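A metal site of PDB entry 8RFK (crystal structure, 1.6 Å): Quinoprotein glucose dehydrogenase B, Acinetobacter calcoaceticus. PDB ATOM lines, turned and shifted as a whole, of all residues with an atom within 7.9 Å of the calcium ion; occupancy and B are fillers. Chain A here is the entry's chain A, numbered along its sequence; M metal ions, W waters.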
ATOM      1  N   SER A 250     -16.117  22.090 -31.364  1.00  0.00           N
ATOM      2  CA  SER A 250     -15.754  23.294 -32.082  1.00  0.00           C
ATOM      3  C   SER A 250     -14.504  23.855 -31.431  1.00  0.00           C
ATOM      4  O   SER A 250     -14.059  23.380 -30.384  1.00  0.00           O
ATOM      5  CB  SER A 250     -16.880  24.334 -32.031  1.00  0.00           C
ATOM      6  OG  SER A 250     -17.019  24.800 -30.705  1.00  0.00           O
ATOM      7  N   ASP A 251     -13.955  24.893 -32.053  1.00  0.00           N
ATOM      8  CA  ASP A 251     -12.989  25.783 -31.407  1.00  0.00           C
ATOM      9  C   ASP A 251     -11.727  25.067 -30.930  1.00  0.00           C
ATOM     10  O   ASP A 251     -11.246  25.310 -29.821  1.00  0.00           O
ATOM     11  CB  ASP A 251     -13.645  26.537 -30.250  1.00  0.00           C
ATOM     12  CG  ASP A 251     -14.692  27.513 -30.714  1.00  0.00           C
ATOM     13  OD1 ASP A 251     -14.299  28.603 -31.180  1.00  0.00           O
ATOM     14  OD2 ASP A 251     -15.904  27.216 -30.568  1.00  0.00           O
ATOM     15  N   GLU A 253      -7.844  25.361 -31.022  1.00  0.00           N
ATOM     16  CA  GLU A 253      -7.153  26.633 -30.850  1.00  0.00           C
ATOM     17  C   GLU A 253      -5.673  26.574 -31.196  1.00  0.00           C
ATOM     18  O   GLU A 253      -4.991  25.553 -30.985  1.00  0.00           O
ATOM     19  CB  GLU A 253      -7.259  27.137 -29.398  1.00  0.00           C
ATOM     20  CG  GLU A 253      -8.666  27.435 -28.937  1.00  0.00           C
ATOM     21  CD  GLU A 253      -8.728  27.849 -27.486  1.00  0.00           C
ATOM     22  OE1 GLU A 253      -7.736  27.637 -26.766  1.00  0.00           O
ATOM     23  OE2 GLU A 253      -9.782  28.374 -27.066  1.00  0.00           O
ATOM     24  N   ASN A 267     -15.020  27.331 -19.292  1.00  0.00           N
ATOM     25  CA  ASN A 267     -16.047  28.376 -19.362  1.00  0.00           C
ATOM     26  C   ASN A 267     -16.086  29.027 -20.737  1.00  0.00           C
ATOM     27  O   ASN A 267     -17.146  29.517 -21.159  1.00  0.00           O
ATOM     28  CB  ASN A 267     -15.785  29.420 -18.279  1.00  0.00           C
ATOM     29  CG  ASN A 267     -15.941  28.854 -16.891  1.00  0.00           C
ATOM     30  OD1 ASN A 267     -14.989  28.338 -16.310  1.00  0.00           O
ATOM     31  ND2 ASN A 267     -17.151  28.936 -16.344  1.00  0.00           N
ATOM     32  N   VAL A 268     -14.967  29.012 -21.468  1.00  0.00           N
ATOM     33  CA  VAL A 268     -14.878  29.644 -22.781  1.00  0.00           C
ATOM     34  C   VAL A 268     -14.166  28.688 -23.725  1.00  0.00           C
ATOM     35  O   VAL A 268     -13.054  28.240 -23.430  1.00  0.00           O
ATOM     36  CB  VAL A 268     -14.123  30.993 -22.739  1.00  0.00           C
ATOM     37  CG1 VAL A 268     -14.150  31.648 -24.119  1.00  0.00           C
ATOM     38  CG2 VAL A 268     -14.722  31.928 -21.696  1.00  0.00           C
ATOM     39  N   ALA A 269     -14.828  28.324 -24.821  1.00  0.00           N
ATOM     40  CA  ALA A 269     -14.210  27.613 -25.925  1.00  0.00           C
ATOM     41  C   ALA A 269     -13.866  28.611 -27.037  1.00  0.00           C
ATOM     42  O   ALA A 269     -14.764  29.262 -27.585  1.00  0.00           O
ATOM     43  CB  ALA A 269     -15.146  26.517 -26.456  1.00  0.00           C
ATOM     44  N   GLY A 270     -12.581  28.744 -27.351  1.00  0.00           N
ATOM     45  CA  GLY A 270     -12.192  29.677 -28.384  1.00  0.00           C
ATOM     46  C   GLY A 270     -12.326  31.110 -27.900  1.00  0.00           C
ATOM     47  O   GLY A 270     -11.907  31.471 -26.796  1.00  0.00           O
ATOM     48  N   TYR A 271     -12.909  31.962 -28.747  1.00  0.00           N
ATOM     49  CA  TYR A 271     -13.155  33.344 -28.357  1.00  0.00           C
ATOM     50  C   TYR A 271     -14.285  33.392 -27.345  1.00  0.00           C
ATOM     51  O   TYR A 271     -15.116  32.489 -27.253  1.00  0.00           O
ATOM     52  CB  TYR A 271     -13.528  34.191 -29.572  1.00  0.00           C
ATOM     53  CG  TYR A 271     -12.475  34.179 -30.646  1.00  0.00           C
ATOM     54  CD1 TYR A 271     -11.340  34.979 -30.544  1.00  0.00           C
ATOM     55  CD2 TYR A 271     -12.595  33.347 -31.750  1.00  0.00           C
ATOM     56  CE1 TYR A 271     -10.359  34.949 -31.519  1.00  0.00           C
ATOM     57  CE2 TYR A 271     -11.623  33.313 -32.729  1.00  0.00           C
ATOM     58  CZ  TYR A 271     -10.506  34.119 -32.613  1.00  0.00           C
ATOM     59  OH  TYR A 271      -9.548  34.071 -33.576  1.00  0.00           O
ATOM     60  N   LYS A 272     -14.323  34.482 -26.578  1.00  0.00           N
ATOM     61  CA  LYS A 272     -15.455  34.765 -25.690  1.00  0.00           C
ATOM     62  C   LYS A 272     -16.534  35.447 -26.527  1.00  0.00           C
ATOM     63  O   LYS A 272     -16.751  36.664 -26.464  1.00  0.00           O
ATOM     64  CB  LYS A 272     -15.028  35.605 -24.511  1.00  0.00           C
ATOM     65  CG  LYS A 272     -16.031  35.636 -23.383  1.00  0.00           C
ATOM     66  CD  LYS A 272     -15.711  36.717 -22.381  1.00  0.00           C
ATOM     67  CE  LYS A 272     -14.647  36.279 -21.389  1.00  0.00           C
ATOM     68  NZ  LYS A 272     -14.574  37.224 -20.240  1.00  0.00           N
ATOM     69  N   ASP A 273     -17.211  34.640 -27.351  1.00  0.00           N
ATOM     70  CA  ASP A 273     -18.150  35.128 -28.352  1.00  0.00           C
ATOM     71  C   ASP A 273     -19.583  34.624 -28.195  1.00  0.00           C
ATOM     72  O   ASP A 273     -20.458  35.050 -28.958  1.00  0.00           O
ATOM     73  CB  ASP A 273     -17.652  34.772 -29.770  1.00  0.00           C
ATOM     74  CG  ASP A 273     -17.342  33.296 -29.946  1.00  0.00           C
ATOM     75  OD1 ASP A 273     -17.710  32.465 -29.091  1.00  0.00           O
ATOM     76  OD2 ASP A 273     -16.733  32.943 -30.970  1.00  0.00           O
ATOM     77  N   ASP A 274     -19.857  33.745 -27.229  1.00  0.00           N
ATOM     78  CA  ASP A 274     -21.195  33.144 -27.105  1.00  0.00           C
ATOM     79  C   ASP A 274     -21.675  32.542 -28.428  1.00  0.00           C
ATOM     80  O   ASP A 274     -22.868  32.585 -28.745  1.00  0.00           O
ATOM     81  CB  ASP A 274     -22.231  34.153 -26.585  1.00  0.00           C
ATOM     82  CG  ASP A 274     -22.023  34.558 -25.141  1.00  0.00           C
ATOM     83  OD1 ASP A 274     -21.115  34.022 -24.471  1.00  0.00           O
ATOM     84  OD2 ASP A 274     -22.807  35.405 -24.649  1.00  0.00           O
ATOM     85  N   SER A 275     -20.763  31.943 -29.194  1.00  0.00           N
ATOM     86  CA  SER A 275     -21.082  31.466 -30.538  1.00  0.00           C
ATOM     87  C   SER A 275     -20.739  29.981 -30.678  1.00  0.00           C
ATOM     88  O   SER A 275     -19.563  29.626 -30.805  1.00  0.00           O
ATOM     89  CB  SER A 275     -20.340  32.290 -31.585  1.00  0.00           C
ATOM     90  OG  SER A 275     -20.871  32.063 -32.877  1.00  0.00           O
ATOM     91  N   GLY A 276     -21.765  29.126 -30.673  1.00  0.00           N
ATOM     92  CA  GLY A 276     -21.621  27.717 -30.966  1.00  0.00           C
ATOM     93  C   GLY A 276     -21.195  26.852 -29.806  1.00  0.00           C
ATOM     94  O   GLY A 276     -21.012  25.638 -30.002  1.00  0.00           O
ATOM     95  N   TYR A 277     -21.039  27.427 -28.610  1.00  0.00           N
ATOM     96  CA  TYR A 277     -20.654  26.698 -27.412  1.00  0.00           C
ATOM     97  C   TYR A 277     -21.213  27.424 -26.196  1.00  0.00           C
ATOM     98  O   TYR A 277     -21.340  28.645 -26.183  1.00  0.00           O
ATOM     99  CB  TYR A 277     -19.127  26.608 -27.242  1.00  0.00           C
ATOM    100  CG  TYR A 277     -18.659  25.986 -25.926  1.00  0.00           C
ATOM    101  CD1 TYR A 277     -18.591  24.607 -25.760  1.00  0.00           C
ATOM    102  CD2 TYR A 277     -18.289  26.791 -24.850  1.00  0.00           C
ATOM    103  CE1 TYR A 277     -18.159  24.041 -24.562  1.00  0.00           C
ATOM    104  CE2 TYR A 277     -17.851  26.238 -23.649  1.00  0.00           C
ATOM    105  CZ  TYR A 277     -17.789  24.855 -23.518  1.00  0.00           C
ATOM    106  OH  TYR A 277     -17.359  24.309 -22.330  1.00  0.00           O
ATOM    107  N   ALA A 278     -21.527  26.641 -25.163  1.00  0.00           N
ATOM    108  CA  ALA A 278     -21.794  27.182 -23.840  1.00  0.00           C
ATOM    109  C   ALA A 278     -21.343  26.127 -22.848  1.00  0.00           C
ATOM    110  O   ALA A 278     -21.195  24.947 -23.197  1.00  0.00           O
ATOM    111  CB  ALA A 278     -23.275  27.537 -23.644  1.00  0.00           C
ATOM    112  N   ASN A 296     -22.679  20.621 -27.853  1.00  0.00           N
ATOM    113  CA  ASN A 296     -21.707  21.656 -27.486  1.00  0.00           C
ATOM    114  C   ASN A 296     -22.276  22.661 -26.490  1.00  0.00           C
ATOM    115  O   ASN A 296     -21.810  23.803 -26.411  1.00  0.00           O
ATOM    116  CB  ASN A 296     -21.166  22.375 -28.723  1.00  0.00           C
ATOM    117  CG  ASN A 296     -19.651  22.526 -28.691  1.00  0.00           C
ATOM    118  OD1 ASN A 296     -18.939  21.657 -28.172  1.00  0.00           O
ATOM    119  ND2 ASN A 296     -19.152  23.613 -29.264  1.00  0.00           N
ATOM    120  N   GLU A 309     -20.481  31.966 -22.236  1.00  0.00           N
ATOM    121  CA  GLU A 309     -19.101  32.423 -22.159  1.00  0.00           C
ATOM    122  C   GLU A 309     -19.012  33.829 -21.563  1.00  0.00           C
ATOM    123  O   GLU A 309     -18.131  34.122 -20.750  1.00  0.00           O
ATOM    124  CB  GLU A 309     -18.489  32.378 -23.558  1.00  0.00           C
ATOM    125  CG  GLU A 309     -18.428  30.949 -24.115  1.00  0.00           C
ATOM    126  CD  GLU A 309     -17.773  30.867 -25.479  1.00  0.00           C
ATOM    127  OE1 GLU A 309     -18.016  31.776 -26.310  1.00  0.00           O
ATOM    128  OE2 GLU A 309     -17.040  29.880 -25.721  1.00  0.00           O
ATOM    129  N   PHE A 317      -8.068  36.266 -18.759  1.00  0.00           N
ATOM    130  CA  PHE A 317      -8.497  35.470 -19.891  1.00  0.00           C
ATOM    131  C   PHE A 317      -7.763  35.902 -21.159  1.00  0.00           C
ATOM    132  O   PHE A 317      -7.810  37.075 -21.550  1.00  0.00           O
ATOM    133  CB  PHE A 317     -10.001  35.573 -20.148  1.00  0.00           C
ATOM    134  CG  PHE A 317     -10.398  34.936 -21.450  1.00  0.00           C
ATOM    135  CD1 PHE A 317     -10.182  33.585 -21.665  1.00  0.00           C
ATOM    136  CD2 PHE A 317     -10.924  35.702 -22.486  1.00  0.00           C
ATOM    137  CE1 PHE A 317     -10.505  32.987 -22.879  1.00  0.00           C
ATOM    138  CE2 PHE A 317     -11.251  35.113 -23.700  1.00  0.00           C
ATOM    139  CZ  PHE A 317     -11.051  33.758 -23.901  1.00  0.00           C
ATOM    140  N   PRO A 320      -7.600  32.856 -28.122  1.00  0.00           N
ATOM    141  CA  PRO A 320      -6.704  32.231 -29.093  1.00  0.00           C
ATOM    142  C   PRO A 320      -6.313  33.148 -30.247  1.00  0.00           C
ATOM    143  O   PRO A 320      -7.038  34.073 -30.624  1.00  0.00           O
ATOM    144  CB  PRO A 320      -7.534  31.044 -29.609  1.00  0.00           C
ATOM    145  CG  PRO A 320      -8.951  31.522 -29.474  1.00  0.00           C
ATOM    146  CD  PRO A 320      -8.988  32.384 -28.247  1.00  0.00           C
ATOM    147  N   THR A 323      -8.882  30.020 -34.290  1.00  0.00           N
ATOM    148  CA  THR A 323      -9.712  28.866 -33.978  1.00  0.00           C
ATOM    149  C   THR A 323      -9.937  28.024 -35.225  1.00  0.00           C
ATOM    150  O   THR A 323     -10.151  28.561 -36.324  1.00  0.00           O
ATOM    151  CB  THR A 323     -11.080  29.256 -33.418  1.00  0.00           C
ATOM    152  OG1 THR A 323     -11.734  30.155 -34.322  1.00  0.00           O
ATOM    153  CG2 THR A 323     -10.937  29.909 -32.046  1.00  0.00           C
ATOM    154  N   THR A 326     -14.723  28.139 -35.638  1.00  0.00           N
ATOM    155  CA  THR A 326     -15.792  28.772 -34.879  1.00  0.00           C
ATOM    156  C   THR A 326     -17.027  28.866 -35.764  1.00  0.00           C
ATOM    157  O   THR A 326     -16.924  29.247 -36.939  1.00  0.00           O
ATOM    158  CB  THR A 326     -15.384  30.158 -34.392  1.00  0.00           C
ATOM    159  OG1 THR A 326     -14.234  30.025 -33.546  1.00  0.00           O
ATOM    160  CG2 THR A 326     -16.502  30.819 -33.597  1.00  0.00           C
ATOM    161  N   VAL A 327     -18.178  28.516 -35.195  1.00  0.00           N
ATOM    162  CA  VAL A 327     -19.441  28.515 -35.914  1.00  0.00           C
ATOM    163  C   VAL A 327     -20.488  29.293 -35.113  1.00  0.00           C
ATOM    164  O   VAL A 327     -20.288  29.659 -33.959  1.00  0.00           O
ATOM    165  CB  VAL A 327     -19.949  27.086 -36.197  1.00  0.00           C
ATOM    166  CG1 VAL A 327     -18.971  26.321 -37.112  1.00  0.00           C
ATOM    167  CG2 VAL A 327     -20.165  26.338 -34.893  1.00  0.00           C
HETATM  168 CA    CA M   1     -16.460  30.791 -27.947  1.00  0.00          CA
HETATM  169  O   HOH W   1     -15.198  30.965 -30.156  1.00  0.00           O
HETATM  170  O   HOH W   2     -17.585  28.995 -29.059  1.00  0.00           O
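N of Ser 275 sits close to OD1 of Asp 273.
The backbone NH (N) of Glu 309 sits at hydrogen-bond distance from the side-chain carboxylate (OD1) of Asp 274.
The calcium ion is bound by the backbone carbonyl oxygen (O) of Tyr 271, the backbone carbonyl oxygen (O) of Ala 269, the side-chain carboxylate (OD1) of Asp 273, water W2, the side-chain carboxylate (OE1) of Glu 309, the side-chain carboxylate (OE2) of Glu 309 and water W1.
Water W1 lies within hydrogen-bond range of the side-chain carboxylate (OD2) of Asp 273, the side-chain carboxylate (OD1) of Asp 251 and the backbone NH (N) of Tyr 271.
Water W2 bridges O of Ser 275 (2.7 Å) and OD2 of Asp 251 (2.9 Å).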
